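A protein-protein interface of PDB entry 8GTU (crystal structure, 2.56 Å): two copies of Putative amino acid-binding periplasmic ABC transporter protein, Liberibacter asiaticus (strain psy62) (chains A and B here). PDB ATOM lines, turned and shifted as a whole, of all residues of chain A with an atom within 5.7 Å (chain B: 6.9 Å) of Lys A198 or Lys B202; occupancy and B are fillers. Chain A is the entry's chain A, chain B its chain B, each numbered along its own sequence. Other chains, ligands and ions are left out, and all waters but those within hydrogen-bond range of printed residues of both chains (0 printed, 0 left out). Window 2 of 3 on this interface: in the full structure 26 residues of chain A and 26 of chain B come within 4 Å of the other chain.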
ATOM      1  N   GLN A  83     -29.522  29.236  16.582  1.00  0.00           N
ATOM      2  CA  GLN A  83     -28.511  29.813  15.707  1.00  0.00           C
ATOM      3  C   GLN A  83     -27.121  29.544  16.276  1.00  0.00           C
ATOM      4  O   GLN A  83     -26.165  29.321  15.533  1.00  0.00           O
ATOM      5  CB  GLN A  83     -28.746  31.307  15.472  1.00  0.00           C
ATOM      6  CG  GLN A  83     -29.413  31.617  14.135  1.00  0.00           C
ATOM      7  CD  GLN A  83     -29.545  33.101  13.894  1.00  0.00           C
ATOM      8  OE1 GLN A  83     -29.587  33.899  14.829  1.00  0.00           O
ATOM      9  NE2 GLN A  83     -29.620  33.490  12.634  1.00  0.00           N
ATOM     10  N   LYS A  84     -27.049  29.549  17.609  1.00  0.00           N
ATOM     11  CA  LYS A  84     -25.813  29.330  18.330  1.00  0.00           C
ATOM     12  C   LYS A  84     -25.323  27.901  18.111  1.00  0.00           C
ATOM     13  O   LYS A  84     -24.116  27.672  18.151  1.00  0.00           O
ATOM     14  CB  LYS A  84     -26.024  29.681  19.808  1.00  0.00           C
ATOM     15  CG  LYS A  84     -25.373  30.978  20.282  1.00  0.00           C
ATOM     16  CD  LYS A  84     -23.834  30.833  20.602  1.00  0.00           C
ATOM     17  CE  LYS A  84     -23.163  31.928  21.438  1.00  0.00           C
ATOM     18  NZ  LYS A  84     -21.785  31.616  21.936  1.00  0.00           N
ATOM     19  N   LYS A  85     -26.245  26.959  17.838  1.00  0.00           N
ATOM     20  CA  LYS A  85     -25.938  25.543  17.973  1.00  0.00           C
ATOM     21  C   LYS A  85     -26.045  24.768  16.650  1.00  0.00           C
ATOM     22  O   LYS A  85     -25.514  23.660  16.551  1.00  0.00           O
ATOM     23  CB  LYS A  85     -26.727  24.956  19.150  1.00  0.00           C
ATOM     24  CG  LYS A  85     -26.071  25.147  20.513  1.00  0.00           C
ATOM     25  CD  LYS A  85     -26.985  25.209  21.742  1.00  0.00           C
ATOM     26  CE  LYS A  85     -28.081  24.162  21.811  1.00  0.00           C
ATOM     27  NZ  LYS A  85     -27.548  22.780  21.880  1.00  0.00           N
ATOM     28  N   TYR A  86     -26.705  25.343  15.630  1.00  0.00           N
ATOM     29  CA  TYR A  86     -26.996  24.656  14.373  1.00  0.00           C
ATOM     30  C   TYR A  86     -26.728  25.592  13.194  1.00  0.00           C
ATOM     31  O   TYR A  86     -26.597  26.793  13.410  1.00  0.00           O
ATOM     32  CB  TYR A  86     -28.465  24.198  14.365  1.00  0.00           C
ATOM     33  CG  TYR A  86     -28.772  23.170  15.423  1.00  0.00           C
ATOM     34  CD1 TYR A  86     -28.301  21.871  15.293  1.00  0.00           C
ATOM     35  CD2 TYR A  86     -29.446  23.510  16.589  1.00  0.00           C
ATOM     36  CE1 TYR A  86     -28.529  20.924  16.270  1.00  0.00           C
ATOM     37  CE2 TYR A  86     -29.691  22.571  17.577  1.00  0.00           C
ATOM     38  CZ  TYR A  86     -29.233  21.273  17.413  1.00  0.00           C
ATOM     39  OH  TYR A  86     -29.435  20.300  18.362  1.00  0.00           O
ATOM     40  N   ASP A  87     -26.673  25.044  11.961  1.00  0.00           N
ATOM     41  CA  ASP A  87     -26.672  25.829  10.729  1.00  0.00           C
ATOM     42  C   ASP A  87     -28.091  25.980  10.196  1.00  0.00           C
ATOM     43  O   ASP A  87     -28.845  25.017  10.248  1.00  0.00           O
ATOM     44  CB  ASP A  87     -25.897  25.144   9.604  1.00  0.00           C
ATOM     45  CG  ASP A  87     -24.400  25.414   9.645  1.00  0.00           C
ATOM     46  OD1 ASP A  87     -23.969  26.122  10.607  1.00  0.00           O
ATOM     47  OD2 ASP A  87     -23.665  24.926   8.706  1.00  0.00           O
ATOM     48  N   MET A 196     -29.571  22.221   9.618  1.00  0.00           N
ATOM     49  CA  MET A 196     -28.535  21.205   9.517  1.00  0.00           C
ATOM     50  C   MET A 196     -27.679  21.274  10.777  1.00  0.00           C
ATOM     51  O   MET A 196     -27.733  22.270  11.513  1.00  0.00           O
ATOM     52  CB  MET A 196     -27.593  21.525   8.354  1.00  0.00           C
ATOM     53  CG  MET A 196     -28.045  21.063   6.991  1.00  0.00           C
ATOM     54  SD  MET A 196     -29.389  22.100   6.468  1.00  0.00           S
ATOM     55  CE  MET A 196     -28.487  23.521   5.869  1.00  0.00           C
ATOM     56  N   ARG A 197     -26.841  20.241  10.974  1.00  0.00           N
ATOM     57  CA  ARG A 197     -25.835  20.294  12.016  1.00  0.00           C
ATOM     58  C   ARG A 197     -24.833  21.400  11.687  1.00  0.00           C
ATOM     59  O   ARG A 197     -24.504  21.614  10.515  1.00  0.00           O
ATOM     60  CB  ARG A 197     -25.096  18.955  12.105  1.00  0.00           C
ATOM     61  CG  ARG A 197     -25.755  17.914  12.994  1.00  0.00           C
ATOM     62  CD  ARG A 197     -24.925  16.661  13.192  1.00  0.00           C
ATOM     63  NE  ARG A 197     -24.529  16.025  11.943  1.00  0.00           N
ATOM     64  CZ  ARG A 197     -25.326  15.406  11.065  1.00  0.00           C
ATOM     65  NH1 ARG A 197     -26.635  15.319  11.258  1.00  0.00           N
ATOM     66  NH2 ARG A 197     -24.790  14.882   9.977  1.00  0.00           N
ATOM     67  N   LYS A 198     -24.338  22.092  12.723  1.00  0.00           N
ATOM     68  CA  LYS A 198     -23.178  22.959  12.563  1.00  0.00           C
ATOM     69  C   LYS A 198     -22.011  22.186  11.949  1.00  0.00           C
ATOM     70  O   LYS A 198     -21.804  21.010  12.252  1.00  0.00           O
ATOM     71  CB  LYS A 198     -22.682  23.496  13.903  1.00  0.00           C
ATOM     72  CG  LYS A 198     -23.209  24.871  14.258  1.00  0.00           C
ATOM     73  CD  LYS A 198     -22.222  25.735  14.984  1.00  0.00           C
ATOM     74  CE  LYS A 198     -21.587  25.085  16.193  1.00  0.00           C
ATOM     75  NZ  LYS A 198     -21.147  26.132  17.140  1.00  0.00           N
ATOM     76  N   GLY A 199     -21.255  22.858  11.077  1.00  0.00           N
ATOM     77  CA  GLY A 199     -20.047  22.265  10.531  1.00  0.00           C
ATOM     78  C   GLY A 199     -20.164  21.850   9.066  1.00  0.00           C
ATOM     79  O   GLY A 199     -19.146  21.745   8.384  1.00  0.00           O
ATOM     80  N   ASN A 200     -21.382  21.611   8.573  1.00  0.00           N
ATOM     81  CA  ASN A 200     -21.479  21.289   7.158  1.00  0.00           C
ATOM     82  C   ASN A 200     -21.901  22.532   6.380  1.00  0.00           C
ATOM     83  O   ASN A 200     -23.053  22.667   5.951  1.00  0.00           O
ATOM     84  CB  ASN A 200     -22.299  20.032   6.872  1.00  0.00           C
ATOM     85  CG  ASN A 200     -21.850  19.324   5.608  1.00  0.00           C
ATOM     86  OD1 ASN A 200     -21.431  19.961   4.642  1.00  0.00           O
ATOM     87  ND2 ASN A 200     -21.902  18.002   5.609  1.00  0.00           N
ATOM     88  N   ASP B  87     -19.973  34.149   1.463  1.00  0.00           N
ATOM     89  CA  ASP B  87     -20.928  33.891   2.535  1.00  0.00           C
ATOM     90  C   ASP B  87     -21.851  35.092   2.682  1.00  0.00           C
ATOM     91  O   ASP B  87     -21.389  36.217   2.598  1.00  0.00           O
ATOM     92  CB  ASP B  87     -20.251  33.768   3.898  1.00  0.00           C
ATOM     93  CG  ASP B  87     -19.668  32.402   4.182  1.00  0.00           C
ATOM     94  OD1 ASP B  87     -19.723  31.554   3.274  1.00  0.00           O
ATOM     95  OD2 ASP B  87     -19.143  32.212   5.304  1.00  0.00           O
ATOM     96  N   GLY B 199     -15.848  30.708   3.759  1.00  0.00           N
ATOM     97  CA  GLY B 199     -14.994  30.037   4.732  1.00  0.00           C
ATOM     98  C   GLY B 199     -14.637  30.911   5.934  1.00  0.00           C
ATOM     99  O   GLY B 199     -13.525  30.843   6.464  1.00  0.00           O
ATOM    100  N   ASN B 200     -15.605  31.739   6.332  1.00  0.00           N
ATOM    101  CA  ASN B 200     -15.517  32.753   7.365  1.00  0.00           C
ATOM    102  C   ASN B 200     -16.797  32.562   8.177  1.00  0.00           C
ATOM    103  O   ASN B 200     -17.616  33.470   8.328  1.00  0.00           O
ATOM    104  CB  ASN B 200     -15.407  34.130   6.686  1.00  0.00           C
ATOM    105  CG  ASN B 200     -14.677  35.219   7.448  1.00  0.00           C
ATOM    106  OD1 ASN B 200     -14.492  36.317   6.919  1.00  0.00           O
ATOM    107  ND2 ASN B 200     -14.270  34.948   8.678  1.00  0.00           N
ATOM    108  N   ASN B 201     -16.997  31.307   8.585  1.00  0.00           N
ATOM    109  CA  ASN B 201     -18.303  30.823   8.996  1.00  0.00           C
ATOM    110  C   ASN B 201     -18.617  31.362  10.387  1.00  0.00           C
ATOM    111  O   ASN B 201     -19.777  31.632  10.695  1.00  0.00           O
ATOM    112  CB  ASN B 201     -18.430  29.309   8.818  1.00  0.00           C
ATOM    113  CG  ASN B 201     -18.102  28.841   7.413  1.00  0.00           C
ATOM    114  OD1 ASN B 201     -18.620  29.368   6.432  1.00  0.00           O
ATOM    115  ND2 ASN B 201     -17.211  27.869   7.302  1.00  0.00           N
ATOM    116  N   LYS B 202     -17.559  31.583  11.182  1.00  0.00           N
ATOM    117  CA  LYS B 202     -17.721  32.000  12.562  1.00  0.00           C
ATOM    118  C   LYS B 202     -18.287  33.415  12.606  1.00  0.00           C
ATOM    119  O   LYS B 202     -19.209  33.693  13.362  1.00  0.00           O
ATOM    120  CB  LYS B 202     -16.417  31.856  13.351  1.00  0.00           C
ATOM    121  CG  LYS B 202     -16.557  31.724  14.868  1.00  0.00           C
ATOM    122  CD  LYS B 202     -17.042  30.346  15.392  1.00  0.00           C
ATOM    123  CE  LYS B 202     -18.522  30.225  15.724  1.00  0.00           C
ATOM    124  NZ  LYS B 202     -18.942  28.816  15.919  1.00  0.00           N
ATOM    125  N   LEU B 203     -17.745  34.296  11.767  1.00  0.00           N
ATOM    126  CA  LEU B 203     -18.211  35.667  11.724  1.00  0.00           C
ATOM    127  C   LEU B 203     -19.643  35.703  11.190  1.00  0.00           C
ATOM    128  O   LEU B 203     -20.450  36.519  11.627  1.00  0.00           O
ATOM    129  CB  LEU B 203     -17.241  36.490  10.870  1.00  0.00           C
ATOM    130  CG  LEU B 203     -17.656  37.923  10.528  1.00  0.00           C
ATOM    131  CD1 LEU B 203     -17.842  38.759  11.799  1.00  0.00           C
ATOM    132  CD2 LEU B 203     -16.624  38.553   9.586  1.00  0.00           C
ATOM    133  N   THR B 204     -19.955  34.801  10.253  1.00  0.00           N
ATOM    134  CA  THR B 204     -21.283  34.751   9.668  1.00  0.00           C
ATOM    135  C   THR B 204     -22.313  34.373  10.737  1.00  0.00           C
ATOM    136  O   THR B 204     -23.353  35.024  10.831  1.00  0.00           O
ATOM    137  CB  THR B 204     -21.274  33.900   8.389  1.00  0.00           C
ATOM    138  OG1 THR B 204     -20.343  34.515   7.504  1.00  0.00           O
ATOM    139  CG2 THR B 204     -22.611  33.826   7.688  1.00  0.00           C
ATOM    140  N   ARG B 205     -22.025  33.323  11.515  1.00  0.00           N
ATOM    141  CA  ARG B 205     -22.934  32.871  12.559  1.00  0.00           C
ATOM    142  C   ARG B 205     -23.141  33.965  13.614  1.00  0.00           C
ATOM    143  O   ARG B 205     -24.264  34.163  14.101  1.00  0.00           O
ATOM    144  CB  ARG B 205     -22.516  31.493  13.083  1.00  0.00           C
ATOM    145  CG  ARG B 205     -22.689  30.401  12.034  1.00  0.00           C
ATOM    146  CD  ARG B 205     -22.558  28.933  12.411  1.00  0.00           C
ATOM    147  NE  ARG B 205     -21.229  28.547  12.871  1.00  0.00           N
ATOM    148  CZ  ARG B 205     -20.330  27.875  12.156  1.00  0.00           C
ATOM    149  NH1 ARG B 205     -20.586  27.524  10.909  1.00  0.00           N
ATOM    150  NH2 ARG B 205     -19.168  27.555  12.699  1.00  0.00           N
ATOM    151  N   SER B 206     -22.058  34.703  13.921  1.00  0.00           N
ATOM    152  CA  SER B 206     -22.069  35.746  14.939  1.00  0.00           C
ATOM    153  C   SER B 206     -22.982  36.905  14.538  1.00  0.00           C
ATOM    154  O   SER B 206     -23.795  37.363  15.351  1.00  0.00           O
ATOM    155  CB  SER B 206     -20.675  36.225  15.217  1.00  0.00           C
ATOM    156  OG  SER B 206     -19.930  35.199  15.863  1.00  0.00           O
ATOM    157  N   ILE B 207     -22.827  37.374  13.286  1.00  0.00           N
ATOM    158  CA  ILE B 207     -23.645  38.453  12.759  1.00  0.00           C
ATOM    159  C   ILE B 207     -25.113  38.032  12.845  1.00  0.00           C
ATOM    160  O   ILE B 207     -25.966  38.822  13.255  1.00  0.00           O
ATOM    161  CB  ILE B 207     -23.176  38.877  11.348  1.00  0.00           C
ATOM    162  CG1 ILE B 207     -21.788  39.518  11.392  1.00  0.00           C
ATOM    163  CG2 ILE B 207     -24.152  39.831  10.671  1.00  0.00           C
ATOM    164  CD1 ILE B 207     -21.244  39.926  10.016  1.00  0.00           C
ATOM    165  N   GLU B 209     -26.605  35.717  14.777  1.00  0.00           N
ATOM    166  CA  GLU B 209     -26.981  35.713  16.176  1.00  0.00           C
ATOM    167  C   GLU B 209     -27.400  37.117  16.593  1.00  0.00           C
ATOM    168  O   GLU B 209     -28.476  37.307  17.164  1.00  0.00           O
ATOM    169  CB  GLU B 209     -25.769  35.265  16.981  1.00  0.00           C
ATOM    170  CG  GLU B 209     -25.727  33.750  17.125  1.00  0.00           C
ATOM    171  CD  GLU B 209     -24.367  33.098  17.345  1.00  0.00           C
ATOM    172  OE1 GLU B 209     -24.267  31.849  17.204  1.00  0.00           O
ATOM    173  OE2 GLU B 209     -23.397  33.828  17.648  1.00  0.00           O
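Positions printed for both chains: 87, 199 and 200. Of the 5 pairs that touch across the chains among the printed residues, none has its exchanged pair printed and touching as well.
Of the printed residues of chain B, Gln A83 touches Glu B209. Printed residues of chain B within 4 Å of Asp A87: Arg B205 (3.6 Å). Printed residues of chain B within 4 Å of Lys A198: Lys B202 (3.7 Å) and Arg B205 (3.7 Å). Lys B202 touches just one residue of chain A: Lys A198. Printed residues of chain A within 4 Å of Glu B209: Gln A83 (3.4 Å) and Lys A84 (3.2 Å). The nearest printed residue of chain B that does not touch Lys A198 is Glu B209 (6.5 Å). The nearest printed residue of chain A that does not touch Arg B205 is Tyr A86 (4.7 Å).
Among the printed residues, pairs that only touch across the chains: Lys A84 with Glu B209, Lys A198 with Lys B202 and Lys A198 with Arg B205.
O of Lys A84 is in hydrogen-bond range of NZ of Lys A198 (3.5 Å). The backbone carbonyl oxygen (O) of Lys B202 lies within hydrogen-bond range of the side-chain hydroxyl (OG) of Ser B206 (3.0 Å). O of Asp A87 sits at hydrogen-bond distance from N of Met A196 (3.0 Å).
Of the 11 printed residues of chain B, 3 touch a printed residue of chain A. Printed residues of chain B that touch a printed residue of chain A: Lys B202, Arg B205 and Glu B209.
NH1 of Arg B205 is in salt-bridge range of OD1 of Asp A87, at 3.7 Å. N of Glu B209 sits close to OE1 of Gln A83, 3.5 Å away.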
